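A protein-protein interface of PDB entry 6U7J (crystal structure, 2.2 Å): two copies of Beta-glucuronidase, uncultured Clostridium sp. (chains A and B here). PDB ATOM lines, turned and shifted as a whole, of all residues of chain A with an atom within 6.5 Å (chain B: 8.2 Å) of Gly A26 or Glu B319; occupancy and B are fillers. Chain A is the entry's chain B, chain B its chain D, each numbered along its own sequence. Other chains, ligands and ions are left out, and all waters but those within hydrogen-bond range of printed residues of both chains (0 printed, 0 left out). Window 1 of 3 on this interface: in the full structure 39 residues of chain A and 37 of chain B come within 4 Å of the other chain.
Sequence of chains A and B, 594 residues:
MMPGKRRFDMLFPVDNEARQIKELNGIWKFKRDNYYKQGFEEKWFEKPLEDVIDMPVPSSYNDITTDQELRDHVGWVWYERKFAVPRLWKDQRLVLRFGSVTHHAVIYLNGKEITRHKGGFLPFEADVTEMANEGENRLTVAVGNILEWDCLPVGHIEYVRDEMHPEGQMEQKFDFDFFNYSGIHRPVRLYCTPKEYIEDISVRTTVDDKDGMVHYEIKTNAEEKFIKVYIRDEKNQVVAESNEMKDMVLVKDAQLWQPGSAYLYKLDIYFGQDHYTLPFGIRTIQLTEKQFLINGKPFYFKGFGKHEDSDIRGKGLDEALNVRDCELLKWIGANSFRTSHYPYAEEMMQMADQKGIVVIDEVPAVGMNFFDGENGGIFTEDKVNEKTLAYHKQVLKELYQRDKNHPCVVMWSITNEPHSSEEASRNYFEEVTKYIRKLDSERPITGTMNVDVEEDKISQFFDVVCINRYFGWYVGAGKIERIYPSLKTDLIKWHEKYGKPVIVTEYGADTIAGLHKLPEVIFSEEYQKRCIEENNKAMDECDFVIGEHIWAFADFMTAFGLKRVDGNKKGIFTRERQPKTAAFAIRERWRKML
NH2 of Arg A313 is in salt-bridge range of OD1 of Asp B318 (2.7 Å).
O of Gly A26 lies within hydrogen-bond range of N of Val A57, at 3.0 Å.
The guanidinium group (NH1) of Arg B313 is in salt-bridge range of the side-chain carboxylate (OD2) of Asp B318, at 3.3 Å.
N of Ala B320 is in hydrogen-bond range of OD1 of Asp B318 (3.0 Å).
The side-chain carboxylate of Asp B318 lies within hydrogen-bond range of the backbone NH of Leu B321 (3.2 Å).
OD1 of Asn B322 sits close to O of Asp B318 (3.4 Å).
Among the printed residues, merely in contact across the chains: Ile A27 with Met B351 (3.6 Å), Gly A26 with Glu B319 (3.6 Å), Pro A56 with Ala B320 (3.6 Å), Ile A27 with Val B323 (3.7 Å), Ile A27 with Glu B319 (3.7 Å), Arg A313 with Ala B320 (3.8 Å) and Pro A56 with Val B323 (3.8 Å).
Positions printed for both chains: 58 and 313.
Of the 8 pairs that touch across the chains among the printed residues, none has its exchanged pair printed and touching as well.
Of the 23 printed residues of chain B, 5 touch a printed residue of chain A.
Of the 11 printed residues of chain A, 4 touch a printed residue of chain B.
Printed residues of chain A that touch a printed residue of chain B: Gly A26, Ile A27, Pro A56 and Arg A313.
Hydrophobic or aromatic side chains of chain A that line the printed part of chain B: Ile A27 and Pro A56.
Along chain A the printed residues that touch a printed residue of chain B span positions 26 to 313.
Among the printed residues, 8 pairs touch across the chains.
Of chain B, only Glu B319 comes within 4 Å of Gly A26.
Of the printed residues of chain B, Arg A313 touches Asp B318 (2.7 Å) and Ala B320 (3.8 Å).
Of the printed residues of chain A, Asp B318 touches Arg A313 (2.7 Å).
Of chain A, only Gly A26 (3.6 Å) and Ile A27 (3.7 Å) come within 4 Å of Glu B319.
Printed residues of chain A within 4 Å of Ala B320: Pro A56 (3.6 Å) and Arg A313 (3.8 Å).
Arg B324 touches none of the printed residues of chain A.
Glu B347 touches none of the printed residues of chain A.
The nearest residue of chain A that does not touch Glu B319 is Pro A56 (4.4 Å).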
ATOM      1  N   LEU A  24      14.938  12.041   9.901  1.00  0.00           N
ATOM      2  CA  LEU A  24      15.269  11.423  11.166  1.00  0.00           C
ATOM      3  C   LEU A  24      16.297  12.240  11.948  1.00  0.00           C
ATOM      4  O   LEU A  24      17.342  11.709  12.337  1.00  0.00           O
ATOM      5  CB  LEU A  24      15.802   9.995  10.949  1.00  0.00           C
ATOM      6  CG  LEU A  24      14.873   9.107  10.125  1.00  0.00           C
ATOM      7  CD1 LEU A  24      15.516   7.756   9.916  1.00  0.00           C
ATOM      8  CD2 LEU A  24      13.525   8.980  10.814  1.00  0.00           C
ATOM      9  N   ASN A  25      16.026  13.512  12.196  1.00  0.00           N
ATOM     10  CA  ASN A  25      16.970  14.393  12.872  1.00  0.00           C
ATOM     11  C   ASN A  25      16.557  14.514  14.348  1.00  0.00           C
ATOM     12  O   ASN A  25      16.352  13.471  14.973  1.00  0.00           O
ATOM     13  CB  ASN A  25      17.073  15.704  12.100  1.00  0.00           C
ATOM     14  CG  ASN A  25      17.521  15.483  10.672  1.00  0.00           C
ATOM     15  OD1 ASN A  25      18.417  14.677  10.404  1.00  0.00           O
ATOM     16  ND2 ASN A  25      16.884  16.169   9.749  1.00  0.00           N
ATOM     17  N   GLY A  26      16.455  15.702  14.927  1.00  0.00           N
ATOM     18  CA  GLY A  26      16.010  15.782  16.302  1.00  0.00           C
ATOM     19  C   GLY A  26      17.097  15.368  17.283  1.00  0.00           C
ATOM     20  O   GLY A  26      18.294  15.559  17.052  1.00  0.00           O
ATOM     21  N   ILE A  27      16.672  14.786  18.397  1.00  0.00           N
ATOM     22  CA  ILE A  27      17.575  14.422  19.478  1.00  0.00           C
ATOM     23  C   ILE A  27      17.742  12.906  19.457  1.00  0.00           C
ATOM     24  O   ILE A  27      16.749  12.170  19.490  1.00  0.00           O
ATOM     25  CB  ILE A  27      17.039  14.905  20.833  1.00  0.00           C
ATOM     26  CG1 ILE A  27      16.726  16.404  20.782  1.00  0.00           C
ATOM     27  CG2 ILE A  27      18.006  14.578  21.921  1.00  0.00           C
ATOM     28  CD1 ILE A  27      17.871  17.263  20.318  1.00  0.00           C
ATOM     29  N   TRP A  28      18.988  12.440  19.374  1.00  0.00           N
ATOM     30  CA  TRP A  28      19.327  11.025  19.441  1.00  0.00           C
ATOM     31  C   TRP A  28      19.958  10.705  20.789  1.00  0.00           C
ATOM     32  O   TRP A  28      20.381  11.598  21.532  1.00  0.00           O
ATOM     33  CB  TRP A  28      20.320  10.635  18.339  1.00  0.00           C
ATOM     34  CG  TRP A  28      19.850  10.767  16.917  1.00  0.00           C
ATOM     35  CD1 TRP A  28      19.115  11.781  16.374  1.00  0.00           C
ATOM     36  CD2 TRP A  28      20.117   9.844  15.853  1.00  0.00           C
ATOM     37  NE1 TRP A  28      18.906  11.542  15.028  1.00  0.00           N
ATOM     38  CE2 TRP A  28      19.515  10.362  14.687  1.00  0.00           C
ATOM     39  CE3 TRP A  28      20.812   8.629  15.777  1.00  0.00           C
ATOM     40  CZ2 TRP A  28      19.575   9.705  13.459  1.00  0.00           C
ATOM     41  CZ3 TRP A  28      20.877   7.984  14.563  1.00  0.00           C
ATOM     42  CH2 TRP A  28      20.263   8.524  13.414  1.00  0.00           C
ATOM     43  N   MET A  55      21.933  13.966  22.141  1.00  0.00           N
ATOM     44  CA  MET A  55      22.812  14.587  21.181  1.00  0.00           C
ATOM     45  C   MET A  55      21.990  15.001  19.964  1.00  0.00           C
ATOM     46  O   MET A  55      21.246  14.169  19.421  1.00  0.00           O
ATOM     47  CB  MET A  55      23.956  13.660  20.755  1.00  0.00           C
ATOM     48  CG  MET A  55      25.035  14.357  19.893  1.00  0.00           C
ATOM     49  SD  MET A  55      26.024  15.618  20.780  1.00  0.00           S
ATOM     50  CE  MET A  55      26.641  14.742  22.200  1.00  0.00           C
ATOM     51  N   PRO A  56      22.080  16.254  19.536  1.00  0.00           N
ATOM     52  CA  PRO A  56      21.314  16.693  18.364  1.00  0.00           C
ATOM     53  C   PRO A  56      21.915  16.165  17.076  1.00  0.00           C
ATOM     54  O   PRO A  56      23.122  15.919  16.977  1.00  0.00           O
ATOM     55  CB  PRO A  56      21.409  18.226  18.419  1.00  0.00           C
ATOM     56  CG  PRO A  56      22.701  18.497  19.184  1.00  0.00           C
ATOM     57  CD  PRO A  56      22.813  17.361  20.190  1.00  0.00           C
ATOM     58  N   VAL A  57      21.048  16.007  16.078  1.00  0.00           N
ATOM     59  CA  VAL A  57      21.430  15.624  14.724  1.00  0.00           C
ATOM     60  C   VAL A  57      20.634  16.510  13.774  1.00  0.00           C
ATOM     61  O   VAL A  57      19.405  16.582  13.898  1.00  0.00           O
ATOM     62  CB  VAL A  57      21.164  14.132  14.458  1.00  0.00           C
ATOM     63  CG1 VAL A  57      21.362  13.807  12.975  1.00  0.00           C
ATOM     64  CG2 VAL A  57      22.067  13.268  15.303  1.00  0.00           C
ATOM     65  N   PRO A  58      21.278  17.214  12.824  1.00  0.00           N
ATOM     66  CA  PRO A  58      22.718  17.202  12.564  1.00  0.00           C
ATOM     67  C   PRO A  58      23.504  18.187  13.450  1.00  0.00           C
ATOM     68  O   PRO A  58      22.949  19.209  13.848  1.00  0.00           O
ATOM     69  CB  PRO A  58      22.800  17.618  11.094  1.00  0.00           C
ATOM     70  CG  PRO A  58      21.633  18.550  10.931  1.00  0.00           C
ATOM     71  CD  PRO A  58      20.556  18.079  11.868  1.00  0.00           C
ATOM     72  N   ARG A  81      18.676   5.988  17.578  1.00  0.00           N
ATOM     73  CA  ARG A  81      17.307   6.466  17.696  1.00  0.00           C
ATOM     74  C   ARG A  81      16.365   5.428  17.099  1.00  0.00           C
ATOM     75  O   ARG A  81      16.789   4.438  16.497  1.00  0.00           O
ATOM     76  CB  ARG A  81      17.122   7.837  17.028  1.00  0.00           C
ATOM     77  CG  ARG A  81      17.146   7.814  15.508  1.00  0.00           C
ATOM     78  CD  ARG A  81      16.508   9.061  14.928  1.00  0.00           C
ATOM     79  NE  ARG A  81      15.050   8.968  14.955  1.00  0.00           N
ATOM     80  CZ  ARG A  81      14.221   9.995  14.788  1.00  0.00           C
ATOM     81  NH1 ARG A  81      14.687  11.227  14.587  1.00  0.00           N
ATOM     82  NH2 ARG A  81      12.921   9.791  14.834  1.00  0.00           N
ATOM     83  N   ARG A 313      27.427  23.995  17.281  1.00  0.00           N
ATOM     84  CA  ARG A 313      27.125  22.812  16.474  1.00  0.00           C
ATOM     85  C   ARG A 313      28.292  22.314  15.626  1.00  0.00           C
ATOM     86  O   ARG A 313      28.108  21.365  14.850  1.00  0.00           O
ATOM     87  CB  ARG A 313      25.941  23.098  15.542  1.00  0.00           C
ATOM     88  CG  ARG A 313      26.271  24.151  14.488  1.00  0.00           C
ATOM     89  CD  ARG A 313      25.114  24.497  13.564  1.00  0.00           C
ATOM     90  NE  ARG A 313      23.799  24.127  14.085  1.00  0.00           N
ATOM     91  CZ  ARG A 313      23.112  24.855  14.956  1.00  0.00           C
ATOM     92  NH1 ARG A 313      23.618  25.986  15.429  1.00  0.00           N
ATOM     93  NH2 ARG A 313      21.920  24.439  15.356  1.00  0.00           N
ATOM     94  N   PHE B  12       0.667  16.618  20.471  1.00  0.00           N
ATOM     95  CA  PHE B  12       1.888  16.774  19.693  1.00  0.00           C
ATOM     96  C   PHE B  12       1.925  15.733  18.573  1.00  0.00           C
ATOM     97  O   PHE B  12       1.622  14.560  18.811  1.00  0.00           O
ATOM     98  CB  PHE B  12       3.120  16.628  20.595  1.00  0.00           C
ATOM     99  CG  PHE B  12       4.413  17.012  19.930  1.00  0.00           C
ATOM    100  CD1 PHE B  12       4.761  18.356  19.768  1.00  0.00           C
ATOM    101  CD2 PHE B  12       5.289  16.035  19.466  1.00  0.00           C
ATOM    102  CE1 PHE B  12       5.964  18.725  19.155  1.00  0.00           C
ATOM    103  CE2 PHE B  12       6.490  16.392  18.852  1.00  0.00           C
ATOM    104  CZ  PHE B  12       6.824  17.750  18.695  1.00  0.00           C
ATOM    105  N   GLU B  23       7.753  17.275   7.459  1.00  0.00           N
ATOM    106  CA  GLU B  23       8.306  18.547   7.907  1.00  0.00           C
ATOM    107  C   GLU B  23       8.350  19.518   6.739  1.00  0.00           C
ATOM    108  O   GLU B  23       8.810  19.162   5.651  1.00  0.00           O
ATOM    109  CB  GLU B  23       9.713  18.344   8.473  1.00  0.00           C
ATOM    110  CG  GLU B  23       9.816  17.241   9.509  1.00  0.00           C
ATOM    111  CD  GLU B  23       9.720  17.776  10.919  1.00  0.00           C
ATOM    112  OE1 GLU B  23       9.519  19.000  11.055  1.00  0.00           O
ATOM    113  OE2 GLU B  23       9.852  16.990  11.891  1.00  0.00           O
ATOM    114  N   PRO B  58      12.562  27.004  10.585  1.00  0.00           N
ATOM    115  CA  PRO B  58      12.145  28.055  11.522  1.00  0.00           C
ATOM    116  C   PRO B  58      13.246  29.084  11.829  1.00  0.00           C
ATOM    117  O   PRO B  58      14.413  28.713  11.943  1.00  0.00           O
ATOM    118  CB  PRO B  58      11.784  27.261  12.782  1.00  0.00           C
ATOM    119  CG  PRO B  58      12.688  26.084  12.747  1.00  0.00           C
ATOM    120  CD  PRO B  58      12.976  25.778  11.290  1.00  0.00           C
ATOM    121  N   PRO B 187       8.683  24.632  14.068  1.00  0.00           N
ATOM    122  CA  PRO B 187       8.540  23.809  12.857  1.00  0.00           C
ATOM    123  C   PRO B 187       7.128  23.828  12.290  1.00  0.00           C
ATOM    124  O   PRO B 187       6.138  23.930  13.017  1.00  0.00           O
ATOM    125  CB  PRO B 187       8.929  22.407  13.332  1.00  0.00           C
ATOM    126  CG  PRO B 187       9.865  22.658  14.475  1.00  0.00           C
ATOM    127  CD  PRO B 187       9.298  23.872  15.169  1.00  0.00           C
ATOM    128  N   ARG B 189       4.551  21.571  10.087  1.00  0.00           N
ATOM    129  CA  ARG B 189       4.363  20.140   9.858  1.00  0.00           C
ATOM    130  C   ARG B 189       3.040  19.885   9.155  1.00  0.00           C
ATOM    131  O   ARG B 189       1.994  20.380   9.591  1.00  0.00           O
ATOM    132  CB  ARG B 189       4.389  19.347  11.171  1.00  0.00           C
ATOM    133  CG  ARG B 189       5.648  19.510  11.986  1.00  0.00           C
ATOM    134  CD  ARG B 189       5.461  18.954  13.374  1.00  0.00           C
ATOM    135  NE  ARG B 189       6.557  19.335  14.257  1.00  0.00           N
ATOM    136  CZ  ARG B 189       7.658  18.612  14.437  1.00  0.00           C
ATOM    137  NH1 ARG B 189       7.813  17.460  13.792  1.00  0.00           N
ATOM    138  NH2 ARG B 189       8.604  19.042  15.257  1.00  0.00           N
ATOM    139  N   ARG B 313      19.398  33.661  14.226  1.00  0.00           N
ATOM    140  CA  ARG B 313      18.054  33.123  14.038  1.00  0.00           C
ATOM    141  C   ARG B 313      17.008  33.727  14.981  1.00  0.00           C
ATOM    142  O   ARG B 313      15.859  33.274  14.972  1.00  0.00           O
ATOM    143  CB  ARG B 313      18.075  31.606  14.208  1.00  0.00           C
ATOM    144  CG  ARG B 313      18.440  31.196  15.637  1.00  0.00           C
ATOM    145  CD  ARG B 313      18.380  29.706  15.846  1.00  0.00           C
ATOM    146  NE  ARG B 313      18.927  28.980  14.709  1.00  0.00           N
ATOM    147  CZ  ARG B 313      20.227  28.843  14.489  1.00  0.00           C
ATOM    148  NH1 ARG B 313      21.103  29.386  15.324  1.00  0.00           N
ATOM    149  NH2 ARG B 313      20.648  28.166  13.442  1.00  0.00           N
ATOM    150  N   GLY B 316      14.141  31.629  16.742  1.00  0.00           N
ATOM    151  CA  GLY B 316      13.885  30.371  16.059  1.00  0.00           C
ATOM    152  C   GLY B 316      14.361  29.177  16.872  1.00  0.00           C
ATOM    153  O   GLY B 316      15.404  29.214  17.529  1.00  0.00           O
ATOM    154  N   LEU B 317      13.582  28.103  16.814  1.00  0.00           N
ATOM    155  CA  LEU B 317      13.934  26.872  17.508  1.00  0.00           C
ATOM    156  C   LEU B 317      15.269  26.359  17.009  1.00  0.00           C
ATOM    157  O   LEU B 317      15.526  26.339  15.802  1.00  0.00           O
ATOM    158  CB  LEU B 317      12.863  25.810  17.279  1.00  0.00           C
ATOM    159  CG  LEU B 317      13.231  24.413  17.777  1.00  0.00           C
ATOM    160  CD1 LEU B 317      13.257  24.416  19.304  1.00  0.00           C
ATOM    161  CD2 LEU B 317      12.239  23.388  17.247  1.00  0.00           C
ATOM    162  N   ASP B 318      16.125  25.955  17.940  1.00  0.00           N
ATOM    163  CA  ASP B 318      17.415  25.372  17.595  1.00  0.00           C
ATOM    164  C   ASP B 318      17.681  24.299  18.633  1.00  0.00           C
ATOM    165  O   ASP B 318      17.985  24.616  19.790  1.00  0.00           O
ATOM    166  CB  ASP B 318      18.520  26.436  17.581  1.00  0.00           C
ATOM    167  CG  ASP B 318      19.915  25.850  17.330  1.00  0.00           C
ATOM    168  OD1 ASP B 318      20.061  24.608  17.281  1.00  0.00           O
ATOM    169  OD2 ASP B 318      20.872  26.639  17.160  1.00  0.00           O
ATOM    170  N   GLU B 319      17.574  23.037  18.221  1.00  0.00           N
ATOM    171  CA  GLU B 319      17.640  21.951  19.188  1.00  0.00           C
ATOM    172  C   GLU B 319      19.066  21.687  19.659  1.00  0.00           C
ATOM    173  O   GLU B 319      19.255  21.199  20.780  1.00  0.00           O
ATOM    174  CB  GLU B 319      17.003  20.689  18.601  1.00  0.00           C
ATOM    175  CG  GLU B 319      15.482  20.788  18.544  1.00  0.00           C
ATOM    176  CD  GLU B 319      14.810  19.449  18.344  1.00  0.00           C
ATOM    177  OE1 GLU B 319      14.738  18.996  17.185  1.00  0.00           O
ATOM    178  OE2 GLU B 319      14.357  18.850  19.346  1.00  0.00           O
ATOM    179  N   ALA B 320      20.077  22.002  18.844  1.00  0.00           N
ATOM    180  CA  ALA B 320      21.443  21.878  19.341  1.00  0.00           C
ATOM    181  C   ALA B 320      21.714  22.922  20.419  1.00  0.00           C
ATOM    182  O   ALA B 320      22.321  22.617  21.453  1.00  0.00           O
ATOM    183  CB  ALA B 320      22.453  22.002  18.200  1.00  0.00           C
ATOM    184  N   LEU B 321      21.246  24.149  20.198  1.00  0.00           N
ATOM    185  CA  LEU B 321      21.267  25.172  21.238  1.00  0.00           C
ATOM    186  C   LEU B 321      20.553  24.690  22.503  1.00  0.00           C
ATOM    187  O   LEU B 321      21.041  24.894  23.624  1.00  0.00           O
ATOM    188  CB  LEU B 321      20.620  26.437  20.680  1.00  0.00           C
ATOM    189  CG  LEU B 321      20.680  27.808  21.353  1.00  0.00           C
ATOM    190  CD1 LEU B 321      19.679  27.855  22.466  1.00  0.00           C
ATOM    191  CD2 LEU B 321      22.063  28.082  21.874  1.00  0.00           C
ATOM    192  N   ASN B 322      19.406  24.015  22.341  1.00  0.00           N
ATOM    193  CA  ASN B 322      18.678  23.526  23.505  1.00  0.00           C
ATOM    194  C   ASN B 322      19.489  22.490  24.274  1.00  0.00           C
ATOM    195  O   ASN B 322      19.530  22.531  25.508  1.00  0.00           O
ATOM    196  CB  ASN B 322      17.329  22.945  23.082  1.00  0.00           C
ATOM    197  CG  ASN B 322      16.339  24.021  22.680  1.00  0.00           C
ATOM    198  OD1 ASN B 322      16.603  25.222  22.845  1.00  0.00           O
ATOM    199  ND2 ASN B 322      15.188  23.603  22.172  1.00  0.00           N
ATOM    200  N   VAL B 323      20.154  21.563  23.571  1.00  0.00           N
ATOM    201  CA  VAL B 323      20.966  20.561  24.270  1.00  0.00           C
ATOM    202  C   VAL B 323      22.142  21.220  24.998  1.00  0.00           C
ATOM    203  O   VAL B 323      22.472  20.860  26.139  1.00  0.00           O
ATOM    204  CB  VAL B 323      21.451  19.477  23.291  1.00  0.00           C
ATOM    205  CG1 VAL B 323      22.341  18.462  24.027  1.00  0.00           C
ATOM    206  CG2 VAL B 323      20.244  18.764  22.668  1.00  0.00           C
ATOM    207  N   ARG B 324      22.785  22.199  24.359  1.00  0.00           N
ATOM    208  CA  ARG B 324      23.877  22.906  25.020  1.00  0.00           C
ATOM    209  C   ARG B 324      23.391  23.577  26.295  1.00  0.00           C
ATOM    210  O   ARG B 324      24.027  23.467  27.348  1.00  0.00           O
ATOM    211  CB  ARG B 324      24.505  23.920  24.053  1.00  0.00           C
ATOM    212  CG  ARG B 324      25.518  24.887  24.695  1.00  0.00           C
ATOM    213  CD  ARG B 324      26.859  24.226  25.052  1.00  0.00           C
ATOM    214  NE  ARG B 324      27.833  25.198  25.557  1.00  0.00           N
ATOM    215  CZ  ARG B 324      29.001  24.888  26.104  1.00  0.00           C
ATOM    216  NH1 ARG B 324      29.369  23.614  26.228  1.00  0.00           N
ATOM    217  NH2 ARG B 324      29.807  25.851  26.524  1.00  0.00           N
ATOM    218  N   ASP B 325      22.237  24.247  26.227  1.00  0.00           N
ATOM    219  CA  ASP B 325      21.692  24.958  27.393  1.00  0.00           C
ATOM    220  C   ASP B 325      21.414  23.995  28.548  1.00  0.00           C
ATOM    221  O   ASP B 325      21.672  24.322  29.708  1.00  0.00           O
ATOM    222  CB  ASP B 325      20.405  25.711  26.999  1.00  0.00           C
ATOM    223  CG  ASP B 325      20.681  27.038  26.223  1.00  0.00           C
ATOM    224  OD1 ASP B 325      21.856  27.288  25.881  1.00  0.00           O
ATOM    225  OD2 ASP B 325      19.716  27.815  25.945  1.00  0.00           O
ATOM    226  N   CYS B 326      20.861  22.805  28.249  1.00  0.00           N
ATOM    227  CA  CYS B 326      20.623  21.812  29.294  1.00  0.00           C
ATOM    228  C   CYS B 326      21.919  21.279  29.893  1.00  0.00           C
ATOM    229  O   CYS B 326      21.986  21.000  31.090  1.00  0.00           O
ATOM    230  CB  CYS B 326      19.793  20.653  28.736  1.00  0.00           C
ATOM    231  SG  CYS B 326      18.126  21.256  28.423  1.00  0.00           S
ATOM    232  N   ALA B 345       9.039  26.373  22.886  1.00  0.00           N
ATOM    233  CA  ALA B 345       8.747  25.269  21.989  1.00  0.00           C
ATOM    234  C   ALA B 345       8.509  24.004  22.799  1.00  0.00           C
ATOM    235  O   ALA B 345       9.176  23.757  23.807  1.00  0.00           O
ATOM    236  CB  ALA B 345       9.902  25.058  21.008  1.00  0.00           C
ATOM    237  N   GLU B 346       7.548  23.201  22.351  1.00  0.00           N
ATOM    238  CA  GLU B 346       7.280  21.927  23.008  1.00  0.00           C
ATOM    239  C   GLU B 346       8.519  21.053  23.063  1.00  0.00           C
ATOM    240  O   GLU B 346       8.689  20.285  24.014  1.00  0.00           O
ATOM    241  CB  GLU B 346       6.140  21.207  22.285  1.00  0.00           C
ATOM    242  CG  GLU B 346       4.988  22.135  22.004  1.00  0.00           C
ATOM    243  CD  GLU B 346       3.812  21.425  21.414  1.00  0.00           C
ATOM    244  OE1 GLU B 346       3.306  20.523  22.124  1.00  0.00           O
ATOM    245  OE2 GLU B 346       3.400  21.767  20.264  1.00  0.00           O
ATOM    246  N   GLU B 347       9.400  21.157  22.063  1.00  0.00           N
ATOM    247  CA  GLU B 347      10.644  20.394  22.095  1.00  0.00           C
ATOM    248  C   GLU B 347      11.430  20.656  23.377  1.00  0.00           C
ATOM    249  O   GLU B 347      11.990  19.728  23.974  1.00  0.00           O
ATOM    250  CB  GLU B 347      11.492  20.724  20.866  1.00  0.00           C
ATOM    251  CG  GLU B 347      11.041  20.011  19.575  1.00  0.00           C
ATOM    252  CD  GLU B 347       9.955  20.771  18.793  1.00  0.00           C
ATOM    253  OE1 GLU B 347       9.469  21.819  19.283  1.00  0.00           O
ATOM    254  OE2 GLU B 347       9.595  20.321  17.671  1.00  0.00           O
ATOM    255  N   MET B 348      11.478  21.916  23.823  1.00  0.00           N
ATOM    256  CA  MET B 348      12.139  22.235  25.087  1.00  0.00           C
ATOM    257  C   MET B 348      11.401  21.620  26.270  1.00  0.00           C
ATOM    258  O   MET B 348      12.024  21.193  27.250  1.00  0.00           O
ATOM    259  CB  MET B 348      12.246  23.754  25.260  1.00  0.00           C
ATOM    260  CG  MET B 348      13.221  24.194  26.355  1.00  0.00           C
ATOM    261  SD  MET B 348      14.893  23.474  26.289  1.00  0.00           S
ATOM    262  CE  MET B 348      15.783  24.705  27.268  1.00  0.00           C
ATOM    263  N   GLN B 350       9.545  18.853  26.163  1.00  0.00           N
ATOM    264  CA  GLN B 350       9.834  17.425  26.117  1.00  0.00           C
ATOM    265  C   GLN B 350      11.199  17.129  26.714  1.00  0.00           C
ATOM    266  O   GLN B 350      11.354  16.171  27.475  1.00  0.00           O
ATOM    267  CB  GLN B 350       9.757  16.913  24.679  1.00  0.00           C
ATOM    268  CG  GLN B 350       8.348  16.875  24.153  1.00  0.00           C
ATOM    269  CD  GLN B 350       8.275  16.980  22.656  1.00  0.00           C
ATOM    270  OE1 GLN B 350       9.252  16.706  21.957  1.00  0.00           O
ATOM    271  NE2 GLN B 350       7.111  17.385  22.141  1.00  0.00           N
ATOM    272  N   MET B 351      12.196  17.955  26.380  1.00  0.00           N
ATOM    273  CA  MET B 351      13.544  17.799  26.920  1.00  0.00           C
ATOM    274  C   MET B 351      13.567  17.952  28.442  1.00  0.00           C
ATOM    275  O   MET B 351      14.233  17.174  29.136  1.00  0.00           O
ATOM    276  CB  MET B 351      14.471  18.817  26.250  1.00  0.00           C
ATOM    277  CG  MET B 351      15.956  18.553  26.378  1.00  0.00           C
ATOM    278  SD  MET B 351      16.868  19.488  25.116  1.00  0.00           S
ATOM    279  CE  MET B 351      16.863  18.256  23.816  1.00  0.00           C
